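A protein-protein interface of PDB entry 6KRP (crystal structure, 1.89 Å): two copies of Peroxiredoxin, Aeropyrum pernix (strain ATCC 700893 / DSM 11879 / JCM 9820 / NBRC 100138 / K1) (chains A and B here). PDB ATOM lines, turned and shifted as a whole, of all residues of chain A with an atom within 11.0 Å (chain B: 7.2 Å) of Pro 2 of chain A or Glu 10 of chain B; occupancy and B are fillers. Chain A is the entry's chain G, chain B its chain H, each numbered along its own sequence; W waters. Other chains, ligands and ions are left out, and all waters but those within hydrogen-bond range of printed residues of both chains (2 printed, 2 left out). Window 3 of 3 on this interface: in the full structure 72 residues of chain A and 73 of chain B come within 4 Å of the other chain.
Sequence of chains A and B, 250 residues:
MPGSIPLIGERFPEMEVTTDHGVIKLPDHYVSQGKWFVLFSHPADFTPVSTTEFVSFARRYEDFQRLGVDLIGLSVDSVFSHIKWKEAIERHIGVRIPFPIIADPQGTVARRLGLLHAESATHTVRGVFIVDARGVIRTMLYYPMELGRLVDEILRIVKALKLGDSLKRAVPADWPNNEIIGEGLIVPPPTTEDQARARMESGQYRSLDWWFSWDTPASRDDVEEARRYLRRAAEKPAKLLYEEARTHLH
The side-chain hydroxyl of Ser 4 of chain B lies close to the backbone carbonyl oxygen of Gly 3 of chain A, at 3.3 Å. O of Gly 3 of chain A sits at hydrogen-bond distance from N of Ile 5 of chain B (2.4 Å). A ring nitrogen (ND1) of His 117 of chain A lies within hydrogen-bond range of the backbone NH (N) of Ile 8 of chain B (2.9 Å). N of Ala 118 of chain A is in hydrogen-bond range of O of Ile 8 of chain B, 2.9 Å away. The backbone NH of Glu 119 of chain A lies within hydrogen-bond range of the backbone carbonyl oxygen of Ile 8 of chain B, at 3.3 Å. The guanidinium group (NH2) of Arg 138 of chain B is in salt-bridge range of the side-chain carboxylate (OE1) of Glu 146 of chain A (2.9 Å). O of Ile 5 of chain B lies close to N of Pro 2 of chain A, at 3.2 Å. The backbone nitrogen (N) of Pro 2 of chain A lies close to the side-chain carboxylate (OE2) of Glu 10 of chain B (3.4 Å).
A ring nitrogen (NE2) of His 117 of chain A sits at hydrogen-bond distance from the backbone carbonyl oxygen of Gly 114 of chain A, at 3.0 Å. N of Leu 7 of chain B lies within hydrogen-bond range of OE1 of Glu 10 of chain B (3.1 Å). The backbone NH of Gly 9 of chain B lies within hydrogen-bond range of the backbone carbonyl oxygen of Ile 137 of chain B (2.9 Å). O of Glu 10 of chain B lies within hydrogen-bond range of N of Ile 137 of chain B, at 2.9 Å.
Among the printed residues, merely in contact across the chains: Pro 2 of chain A with Leu 7 of chain B, Gly 3 of chain A with Leu 7 of chain B, Ser 4 of chain A with Ser 4 of chain B, Ile 5 of chain A with Ile 5 of chain B, Leu 116 of chain A with Leu 7 of chain B, His 117 of chain A with Leu 7 of chain B, Ala 118 of chain A with Gly 9 of chain B, Ala 118 of chain A with Glu 10 of chain B and Pro 144 of chain A with Arg 138 of chain B.
Printed residues of chain B within 4 Å of Pro 144 of chain A: Arg 138 (3.2 Å). Of the printed residues of chain A, Ile 5 of chain B touches Pro 2, Gly 3 and Ile 5. Leu 7 of chain B touches four residues of chain A. Of the printed residues of chain A, Ile 8 of chain B touches His 117 (2.9 Å), Ala 118 (2.9 Å) and Glu 119 (3.3 Å). Of chain A, only Pro 2 (3.0 Å) and Ala 118 (3.6 Å) come within 4 Å of Glu 10 of chain B. No residue of chain A comes within 4 Å of Val 136 of chain B. The nearest residue of chain A that does not touch Glu 10 of chain B is Gly 3 of chain A (5.4 Å).
Of the 18 printed residues of chain A, 10 touch a printed residue of chain B. Among the printed residues, 17 pairs touch across the chains. Among the printed residues, Asp or Glu carboxylates within 4 Å of a Lys or Arg side-chain nitrogen of the other chain: Glu 146 of chain A with Arg 138 of chain B.
Ser 4 of chain A touches its own counterpart, Ser 4 of chain B. Ile 5 of chain A touches its own counterpart, Ile 5 of chain B. 2 positions are printed for both chains.
Water W2 lies within hydrogen-bond range of N of Gly 9 of chain B (3.3 Å) and OE2 of Glu 119 of chain A (3.4 Å). Water W1 lies within hydrogen-bond range of the side-chain hydroxyl of Ser 4 of chain B (3.3 Å) and the backbone NH of Gly 3 of chain A (3.5 Å).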
ATOM      1  N   PRO A   2      24.393  12.625 -22.282  1.00  0.00           N
ATOM      2  CA  PRO A   2      25.330  11.757 -21.531  1.00  0.00           C
ATOM      3  C   PRO A   2      25.082  10.239 -21.652  1.00  0.00           C
ATOM      4  O   PRO A   2      25.189   9.553 -20.642  1.00  0.00           O
ATOM      5  CB  PRO A   2      25.148  12.257 -20.084  1.00  0.00           C
ATOM      6  CG  PRO A   2      25.044  13.758 -20.261  1.00  0.00           C
ATOM      7  CD  PRO A   2      24.564  13.968 -21.692  1.00  0.00           C
ATOM      8  N   GLY A   3      24.810   9.741 -22.868  1.00  0.00           N
ATOM      9  CA  GLY A   3      24.604   8.299 -23.118  1.00  0.00           C
ATOM     10  C   GLY A   3      24.683   7.912 -24.591  1.00  0.00           C
ATOM     11  O   GLY A   3      24.161   8.687 -25.427  1.00  0.00           O
ATOM     12  N   SER A   4      25.277   6.736 -24.878  1.00  0.00           N
ATOM     13  CA  SER A   4      25.469   6.110 -26.223  1.00  0.00           C
ATOM     14  C   SER A   4      24.457   4.975 -26.445  1.00  0.00           C
ATOM     15  O   SER A   4      23.983   4.421 -25.452  1.00  0.00           O
ATOM     16  CB  SER A   4      26.899   5.611 -26.385  1.00  0.00           C
ATOM     17  OG  SER A   4      27.018   4.704 -27.481  1.00  0.00           O
ATOM     18  N   ILE A   5      24.166   4.623 -27.704  1.00  0.00           N
ATOM     19  CA  ILE A   5      23.233   3.509 -28.067  1.00  0.00           C
ATOM     20  C   ILE A   5      23.784   2.688 -29.245  1.00  0.00           C
ATOM     21  O   ILE A   5      24.760   3.019 -29.913  1.00  0.00           O
ATOM     22  CB  ILE A   5      21.789   4.025 -28.340  1.00  0.00           C
ATOM     23  CG1 ILE A   5      21.767   5.398 -29.024  1.00  0.00           C
ATOM     24  CG2 ILE A   5      20.938   4.018 -27.064  1.00  0.00           C
ATOM     25  CD1 ILE A   5      20.431   5.767 -29.646  1.00  0.00           C
ATOM     26  N   ALA A 110      21.824  -3.212 -19.788  1.00  0.00           N
ATOM     27  CA  ALA A 110      21.238  -1.854 -19.877  1.00  0.00           C
ATOM     28  C   ALA A 110      22.297  -0.834 -20.347  1.00  0.00           C
ATOM     29  O   ALA A 110      21.997   0.030 -21.199  1.00  0.00           O
ATOM     30  CB  ALA A 110      20.618  -1.504 -18.550  1.00  0.00           C
ATOM     31  N   ARG A 111      23.527  -0.924 -19.862  1.00  0.00           N
ATOM     32  CA  ARG A 111      24.568   0.051 -20.262  1.00  0.00           C
ATOM     33  C   ARG A 111      24.905  -0.184 -21.738  1.00  0.00           C
ATOM     34  O   ARG A 111      25.027   0.783 -22.466  1.00  0.00           O
ATOM     35  CB  ARG A 111      25.786  -0.071 -19.335  1.00  0.00           C
ATOM     36  CG  ARG A 111      26.171   1.264 -18.723  1.00  0.00           C
ATOM     37  CD  ARG A 111      27.239   1.156 -17.659  1.00  0.00           C
ATOM     38  NE  ARG A 111      26.558   0.803 -16.428  1.00  0.00           N
ATOM     39  CZ  ARG A 111      26.558  -0.394 -15.832  1.00  0.00           C
ATOM     40  NH1 ARG A 111      27.255  -1.410 -16.331  1.00  0.00           N
ATOM     41  NH2 ARG A 111      25.866  -0.535 -14.705  1.00  0.00           N
ATOM     42  N   LEU A 113      23.031  -1.130 -24.097  1.00  0.00           N
ATOM     43  CA  LEU A 113      21.912  -0.743 -24.993  1.00  0.00           C
ATOM     44  C   LEU A 113      21.491   0.712 -24.746  1.00  0.00           C
ATOM     45  O   LEU A 113      20.548   1.131 -25.394  1.00  0.00           O
ATOM     46  CB  LEU A 113      20.728  -1.699 -24.758  1.00  0.00           C
ATOM     47  CG  LEU A 113      21.002  -3.158 -25.122  1.00  0.00           C
ATOM     48  CD1 LEU A 113      19.756  -3.987 -24.904  1.00  0.00           C
ATOM     49  CD2 LEU A 113      21.476  -3.272 -26.568  1.00  0.00           C
ATOM     50  N   GLY A 114      22.133   1.418 -23.812  1.00  0.00           N
ATOM     51  CA  GLY A 114      21.873   2.858 -23.626  1.00  0.00           C
ATOM     52  C   GLY A 114      20.557   3.095 -22.922  1.00  0.00           C
ATOM     53  O   GLY A 114      19.947   4.122 -23.199  1.00  0.00           O
ATOM     54  N   LEU A 115      20.148   2.180 -22.022  1.00  0.00           N
ATOM     55  CA  LEU A 115      18.779   2.140 -21.428  1.00  0.00           C
ATOM     56  C   LEU A 115      18.756   2.802 -20.040  1.00  0.00           C
ATOM     57  O   LEU A 115      17.671   2.923 -19.456  1.00  0.00           O
ATOM     58  CB  LEU A 115      18.307   0.686 -21.332  1.00  0.00           C
ATOM     59  CG  LEU A 115      17.978  -0.001 -22.666  1.00  0.00           C
ATOM     60  CD1 LEU A 115      17.648  -1.463 -22.435  1.00  0.00           C
ATOM     61  CD2 LEU A 115      16.869   0.730 -23.413  1.00  0.00           C
ATOM     62  N   LEU A 116      19.883   3.305 -19.555  1.00  0.00           N
ATOM     63  CA  LEU A 116      19.937   4.124 -18.315  1.00  0.00           C
ATOM     64  C   LEU A 116      19.929   5.599 -18.724  1.00  0.00           C
ATOM     65  O   LEU A 116      20.972   6.127 -19.197  1.00  0.00           O
ATOM     66  CB  LEU A 116      21.217   3.791 -17.536  1.00  0.00           C
ATOM     67  CG  LEU A 116      21.186   2.698 -16.466  1.00  0.00           C
ATOM     68  CD1 LEU A 116      19.904   1.929 -16.397  1.00  0.00           C
ATOM     69  CD2 LEU A 116      22.385   1.753 -16.582  1.00  0.00           C
ATOM     70  N   HIS A 117      18.826   6.300 -18.467  1.00  0.00           N
ATOM     71  CA  HIS A 117      18.677   7.742 -18.769  1.00  0.00           C
ATOM     72  C   HIS A 117      18.682   8.512 -17.458  1.00  0.00           C
ATOM     73  O   HIS A 117      19.027   7.905 -16.422  1.00  0.00           O
ATOM     74  CB  HIS A 117      17.443   7.979 -19.669  1.00  0.00           C
ATOM     75  CG  HIS A 117      17.586   7.455 -21.058  1.00  0.00           C
ATOM     76  ND1 HIS A 117      17.037   8.124 -22.151  1.00  0.00           N
ATOM     77  CD2 HIS A 117      18.217   6.368 -21.565  1.00  0.00           C
ATOM     78  CE1 HIS A 117      17.328   7.461 -23.253  1.00  0.00           C
ATOM     79  NE2 HIS A 117      18.000   6.363 -22.925  1.00  0.00           N
ATOM     80  N   ALA A 118      18.426   9.825 -17.519  1.00  0.00           N
ATOM     81  CA  ALA A 118      18.666  10.751 -16.391  1.00  0.00           C
ATOM     82  C   ALA A 118      17.487  10.729 -15.423  1.00  0.00           C
ATOM     83  O   ALA A 118      17.647  11.214 -14.321  1.00  0.00           O
ATOM     84  CB  ALA A 118      18.933  12.134 -16.918  1.00  0.00           C
ATOM     85  N   GLU A 119      16.334  10.185 -15.809  1.00  0.00           N
ATOM     86  CA  GLU A 119      15.118  10.118 -14.958  1.00  0.00           C
ATOM     87  C   GLU A 119      15.350   9.145 -13.790  1.00  0.00           C
ATOM     88  O   GLU A 119      14.827   9.391 -12.701  1.00  0.00           O
ATOM     89  CB  GLU A 119      13.955   9.735 -15.887  1.00  0.00           C
ATOM     90  CG  GLU A 119      12.600   9.945 -15.302  1.00  0.00           C
ATOM     91  CD  GLU A 119      11.449   9.737 -16.285  1.00  0.00           C
ATOM     92  OE1 GLU A 119      11.457   8.747 -17.046  1.00  0.00           O
ATOM     93  OE2 GLU A 119      10.540  10.513 -16.222  1.00  0.00           O
ATOM     94  N   SER A 120      16.152   8.095 -13.967  1.00  0.00           N
ATOM     95  CA  SER A 120      16.526   7.151 -12.881  1.00  0.00           C
ATOM     96  C   SER A 120      17.960   6.706 -13.063  1.00  0.00           C
ATOM     97  O   SER A 120      18.297   6.292 -14.152  1.00  0.00           O
ATOM     98  CB  SER A 120      15.602   5.945 -12.858  1.00  0.00           C
ATOM     99  OG  SER A 120      16.012   4.992 -11.892  1.00  0.00           O
ATOM    100  N   ALA A 121      18.751   6.683 -11.985  1.00  0.00           N
ATOM    101  CA  ALA A 121      20.148   6.194 -12.002  1.00  0.00           C
ATOM    102  C   ALA A 121      20.130   4.669 -11.908  1.00  0.00           C
ATOM    103  O   ALA A 121      21.126   4.066 -12.262  1.00  0.00           O
ATOM    104  CB  ALA A 121      20.956   6.803 -10.870  1.00  0.00           C
ATOM    105  N   VAL A 125      14.836   3.017 -18.582  1.00  0.00           N
ATOM    106  CA  VAL A 125      13.682   3.622 -19.294  1.00  0.00           C
ATOM    107  C   VAL A 125      12.863   2.497 -19.959  1.00  0.00           C
ATOM    108  O   VAL A 125      13.190   1.264 -19.780  1.00  0.00           O
ATOM    109  CB  VAL A 125      14.141   4.696 -20.304  1.00  0.00           C
ATOM    110  CG1 VAL A 125      14.874   5.830 -19.611  1.00  0.00           C
ATOM    111  CG2 VAL A 125      14.983   4.104 -21.395  1.00  0.00           C
ATOM    112  N   PRO A 144       9.286   7.069 -21.211  1.00  0.00           N
ATOM    113  CA  PRO A 144       9.746   7.310 -19.853  1.00  0.00           C
ATOM    114  C   PRO A 144       8.999   6.480 -18.801  1.00  0.00           C
ATOM    115  O   PRO A 144       8.042   5.783 -19.121  1.00  0.00           O
ATOM    116  CB  PRO A 144       9.458   8.817 -19.763  1.00  0.00           C
ATOM    117  CG  PRO A 144       8.118   8.954 -20.448  1.00  0.00           C
ATOM    118  CD  PRO A 144       8.233   8.007 -21.626  1.00  0.00           C
ATOM    119  N   GLU A 146       6.918   7.287 -16.561  1.00  0.00           N
ATOM    120  CA  GLU A 146       5.542   7.735 -16.251  1.00  0.00           C
ATOM    121  C   GLU A 146       4.521   7.401 -17.365  1.00  0.00           C
ATOM    122  O   GLU A 146       3.315   7.635 -17.130  1.00  0.00           O
ATOM    123  CB  GLU A 146       5.548   9.219 -15.883  1.00  0.00           C
ATOM    124  CG  GLU A 146       5.970  10.161 -17.001  1.00  0.00           C
ATOM    125  CD  GLU A 146       7.457  10.497 -17.091  1.00  0.00           C
ATOM    126  OE1 GLU A 146       7.761  11.531 -17.690  1.00  0.00           O
ATOM    127  OE2 GLU A 146       8.303   9.719 -16.570  1.00  0.00           O
ATOM    128  N   SER B   4      26.372   8.421 -29.498  1.00  0.00           N
ATOM    129  CA  SER B   4      25.990   9.106 -28.225  1.00  0.00           C
ATOM    130  C   SER B   4      24.692   9.916 -28.398  1.00  0.00           C
ATOM    131  O   SER B   4      24.390  10.281 -29.549  1.00  0.00           O
ATOM    132  CB  SER B   4      27.129   9.965 -27.709  1.00  0.00           C
ATOM    133  OG  SER B   4      26.987  10.204 -26.310  1.00  0.00           O
ATOM    134  N   ILE B   5      23.949  10.186 -27.309  1.00  0.00           N
ATOM    135  CA  ILE B   5      22.675  10.977 -27.357  1.00  0.00           C
ATOM    136  C   ILE B   5      22.470  11.854 -26.113  1.00  0.00           C
ATOM    137  O   ILE B   5      23.101  11.715 -25.051  1.00  0.00           O
ATOM    138  CB  ILE B   5      21.416  10.098 -27.628  1.00  0.00           C
ATOM    139  CG1 ILE B   5      21.284   8.894 -26.681  1.00  0.00           C
ATOM    140  CG2 ILE B   5      21.335   9.673 -29.096  1.00  0.00           C
ATOM    141  CD1 ILE B   5      19.922   8.208 -26.714  1.00  0.00           C
ATOM    142  N   PRO B   6      21.531  12.820 -26.254  1.00  0.00           N
ATOM    143  CA  PRO B   6      20.764  13.343 -25.127  1.00  0.00           C
ATOM    144  C   PRO B   6      19.904  12.225 -24.510  1.00  0.00           C
ATOM    145  O   PRO B   6      19.570  11.300 -25.224  1.00  0.00           O
ATOM    146  CB  PRO B   6      19.835  14.387 -25.753  1.00  0.00           C
ATOM    147  CG  PRO B   6      20.465  14.720 -27.078  1.00  0.00           C
ATOM    148  CD  PRO B   6      21.128  13.437 -27.527  1.00  0.00           C
ATOM    149  N   LEU B   7      19.517  12.353 -23.240  1.00  0.00           N
ATOM    150  CA  LEU B   7      18.766  11.302 -22.506  1.00  0.00           C
ATOM    151  C   LEU B   7      17.447  11.854 -21.953  1.00  0.00           C
ATOM    152  O   LEU B   7      17.351  13.035 -21.635  1.00  0.00           O
ATOM    153  CB  LEU B   7      19.645  10.758 -21.390  1.00  0.00           C
ATOM    154  CG  LEU B   7      20.982  10.152 -21.810  1.00  0.00           C
ATOM    155  CD1 LEU B   7      21.788   9.735 -20.587  1.00  0.00           C
ATOM    156  CD2 LEU B   7      20.808   8.990 -22.756  1.00  0.00           C
ATOM    157  N   ILE B   8      16.461  10.991 -21.798  1.00  0.00           N
ATOM    158  CA  ILE B   8      15.209  11.335 -21.089  1.00  0.00           C
ATOM    159  C   ILE B   8      15.557  11.870 -19.696  1.00  0.00           C
ATOM    160  O   ILE B   8      16.372  11.227 -18.991  1.00  0.00           O
ATOM    161  CB  ILE B   8      14.248  10.132 -21.039  1.00  0.00           C
ATOM    162  CG1 ILE B   8      13.794   9.737 -22.446  1.00  0.00           C
ATOM    163  CG2 ILE B   8      13.089  10.469 -20.114  1.00  0.00           C
ATOM    164  CD1 ILE B   8      12.956   8.483 -22.505  1.00  0.00           C
ATOM    165  N   GLY B   9      14.944  12.995 -19.289  1.00  0.00           N
ATOM    166  CA  GLY B   9      15.176  13.593 -17.965  1.00  0.00           C
ATOM    167  C   GLY B   9      16.286  14.623 -17.994  1.00  0.00           C
ATOM    168  O   GLY B   9      16.430  15.356 -17.007  1.00  0.00           O
ATOM    169  N   GLU B  10      17.021  14.758 -19.075  1.00  0.00           N
ATOM    170  CA  GLU B  10      18.019  15.855 -19.181  1.00  0.00           C
ATOM    171  C   GLU B  10      17.358  17.057 -19.836  1.00  0.00           C
ATOM    172  O   GLU B  10      16.496  16.885 -20.715  1.00  0.00           O
ATOM    173  CB  GLU B  10      19.221  15.510 -20.051  1.00  0.00           C
ATOM    174  CG  GLU B  10      20.071  14.389 -19.503  1.00  0.00           C
ATOM    175  CD  GLU B  10      21.237  13.980 -20.391  1.00  0.00           C
ATOM    176  OE1 GLU B  10      21.266  14.317 -21.614  1.00  0.00           O
ATOM    177  OE2 GLU B  10      22.100  13.275 -19.847  1.00  0.00           O
ATOM    178  N   ARG B  11      17.892  18.231 -19.538  1.00  0.00           N
ATOM    179  CA  ARG B  11      17.621  19.455 -20.326  1.00  0.00           C
ATOM    180  C   ARG B  11      18.095  19.219 -21.769  1.00  0.00           C
ATOM    181  O   ARG B  11      19.170  18.593 -22.009  1.00  0.00           O
ATOM    182  CB  ARG B  11      18.284  20.687 -19.710  1.00  0.00           C
ATOM    183  CG  ARG B  11      17.640  21.997 -20.155  1.00  0.00           C
ATOM    184  CD  ARG B  11      18.073  23.177 -19.293  1.00  0.00           C
ATOM    185  NE  ARG B  11      17.516  24.464 -19.713  1.00  0.00           N
ATOM    186  CZ  ARG B  11      17.990  25.157 -20.727  1.00  0.00           C
ATOM    187  NH1 ARG B  11      18.978  24.623 -21.434  1.00  0.00           N
ATOM    188  NH2 ARG B  11      17.483  26.345 -21.051  1.00  0.00           N
ATOM    189  N   PHE B  12      17.276  19.637 -22.712  1.00  0.00           N
ATOM    190  CA  PHE B  12      17.648  19.658 -24.143  1.00  0.00           C
ATOM    191  C   PHE B  12      18.919  20.485 -24.288  1.00  0.00           C
ATOM    192  O   PHE B  12      19.019  21.552 -23.711  1.00  0.00           O
ATOM    193  CB  PHE B  12      16.529  20.261 -24.967  1.00  0.00           C
ATOM    194  CG  PHE B  12      16.754  20.160 -26.440  1.00  0.00           C
ATOM    195  CD1 PHE B  12      16.332  19.040 -27.126  1.00  0.00           C
ATOM    196  CD2 PHE B  12      17.428  21.157 -27.122  1.00  0.00           C
ATOM    197  CE1 PHE B  12      16.536  18.935 -28.490  1.00  0.00           C
ATOM    198  CE2 PHE B  12      17.681  21.018 -28.478  1.00  0.00           C
ATOM    199  CZ  PHE B  12      17.172  19.947 -29.166  1.00  0.00           C
ATOM    200  N   PRO B  13      19.943  19.996 -25.000  1.00  0.00           N
ATOM    201  CA  PRO B  13      21.212  20.722 -25.053  1.00  0.00           C
ATOM    202  C   PRO B  13      21.005  22.145 -25.581  1.00  0.00           C
ATOM    203  O   PRO B  13      20.376  22.268 -26.654  1.00  0.00           O
ATOM    204  CB  PRO B  13      22.046  19.912 -26.075  1.00  0.00           C
ATOM    205  CG  PRO B  13      21.378  18.573 -26.224  1.00  0.00           C
ATOM    206  CD  PRO B  13      19.935  18.755 -25.783  1.00  0.00           C
ATOM    207  N   ARG B 112      25.197  16.541 -32.536  1.00  0.00           N
ATOM    208  CA  ARG B 112      24.960  16.898 -31.120  1.00  0.00           C
ATOM    209  C   ARG B 112      23.803  16.020 -30.629  1.00  0.00           C
ATOM    210  O   ARG B 112      23.866  15.587 -29.500  1.00  0.00           O
ATOM    211  CB  ARG B 112      24.685  18.404 -30.968  1.00  0.00           C
ATOM    212  CG  ARG B 112      24.503  18.882 -29.537  1.00  0.00           C
ATOM    213  CD  ARG B 112      25.771  18.693 -28.718  1.00  0.00           C
ATOM    214  NE  ARG B 112      25.733  19.199 -27.357  1.00  0.00           N
ATOM    215  CZ  ARG B 112      25.328  18.512 -26.283  1.00  0.00           C
ATOM    216  NH1 ARG B 112      24.858  17.282 -26.395  1.00  0.00           N
ATOM    217  NH2 ARG B 112      25.349  19.091 -25.093  1.00  0.00           N
ATOM    218  N   VAL B 131       9.885  17.567 -25.861  1.00  0.00           N
ATOM    219  CA  VAL B 131      10.514  18.447 -24.839  1.00  0.00           C
ATOM    220  C   VAL B 131       9.414  19.247 -24.130  1.00  0.00           C
ATOM    221  O   VAL B 131       8.630  19.909 -24.796  1.00  0.00           O
ATOM    222  CB  VAL B 131      11.563  19.375 -25.461  1.00  0.00           C
ATOM    223  CG1 VAL B 131      12.331  20.122 -24.388  1.00  0.00           C
ATOM    224  CG2 VAL B 131      12.518  18.588 -26.334  1.00  0.00           C
ATOM    225  N   GLY B 135      12.017  22.649 -20.709  1.00  0.00           N
ATOM    226  CA  GLY B 135      13.162  22.314 -21.583  1.00  0.00           C
ATOM    227  C   GLY B 135      13.730  20.931 -21.349  1.00  0.00           C
ATOM    228  O   GLY B 135      14.874  20.667 -21.811  1.00  0.00           O
ATOM    229  N   VAL B 136      12.961  20.036 -20.722  1.00  0.00           N
ATOM    230  CA  VAL B 136      13.422  18.656 -20.388  1.00  0.00           C
ATOM    231  C   VAL B 136      12.910  17.686 -21.457  1.00  0.00           C
ATOM    232  O   VAL B 136      11.686  17.711 -21.818  1.00  0.00           O
ATOM    233  CB  VAL B 136      12.977  18.236 -18.967  1.00  0.00           C
ATOM    234  CG1 VAL B 136      13.294  16.774 -18.650  1.00  0.00           C
ATOM    235  CG2 VAL B 136      13.579  19.154 -17.901  1.00  0.00           C
ATOM    236  N   ILE B 137      13.799  16.777 -21.892  1.00  0.00           N
ATOM    237  CA  ILE B 137      13.467  15.697 -22.833  1.00  0.00           C
ATOM    238  C   ILE B 137      12.599  14.674 -22.092  1.00  0.00           C
ATOM    239  O   ILE B 137      13.029  14.157 -21.055  1.00  0.00           O
ATOM    240  CB  ILE B 137      14.752  15.100 -23.430  1.00  0.00           C
ATOM    241  CG1 ILE B 137      15.549  16.145 -24.219  1.00  0.00           C
ATOM    242  CG2 ILE B 137      14.406  13.912 -24.285  1.00  0.00           C
ATOM    243  CD1 ILE B 137      16.964  15.653 -24.638  1.00  0.00           C
ATOM    244  N   ARG B 138      11.430  14.380 -22.641  1.00  0.00           N
ATOM    245  CA  ARG B 138      10.437  13.497 -21.967  1.00  0.00           C
ATOM    246  C   ARG B 138      10.315  12.136 -22.648  1.00  0.00           C
ATOM    247  O   ARG B 138       9.883  11.160 -21.964  1.00  0.00           O
ATOM    248  CB  ARG B 138       9.103  14.238 -21.934  1.00  0.00           C
ATOM    249  CG  ARG B 138       9.112  15.552 -21.156  1.00  0.00           C
ATOM    250  CD  ARG B 138       9.559  15.449 -19.710  1.00  0.00           C
ATOM    251  NE  ARG B 138       8.615  14.635 -18.956  1.00  0.00           N
ATOM    252  CZ  ARG B 138       7.506  15.089 -18.394  1.00  0.00           C
ATOM    253  NH1 ARG B 138       7.227  16.378 -18.446  1.00  0.00           N
ATOM    254  NH2 ARG B 138       6.666  14.250 -17.791  1.00  0.00           N
HETATM  255  O   HOH W   1      27.363  12.010 -23.584  1.00  0.00           O
HETATM  256  O   HOH W   2      12.075  13.137 -17.709  1.00  0.00           O
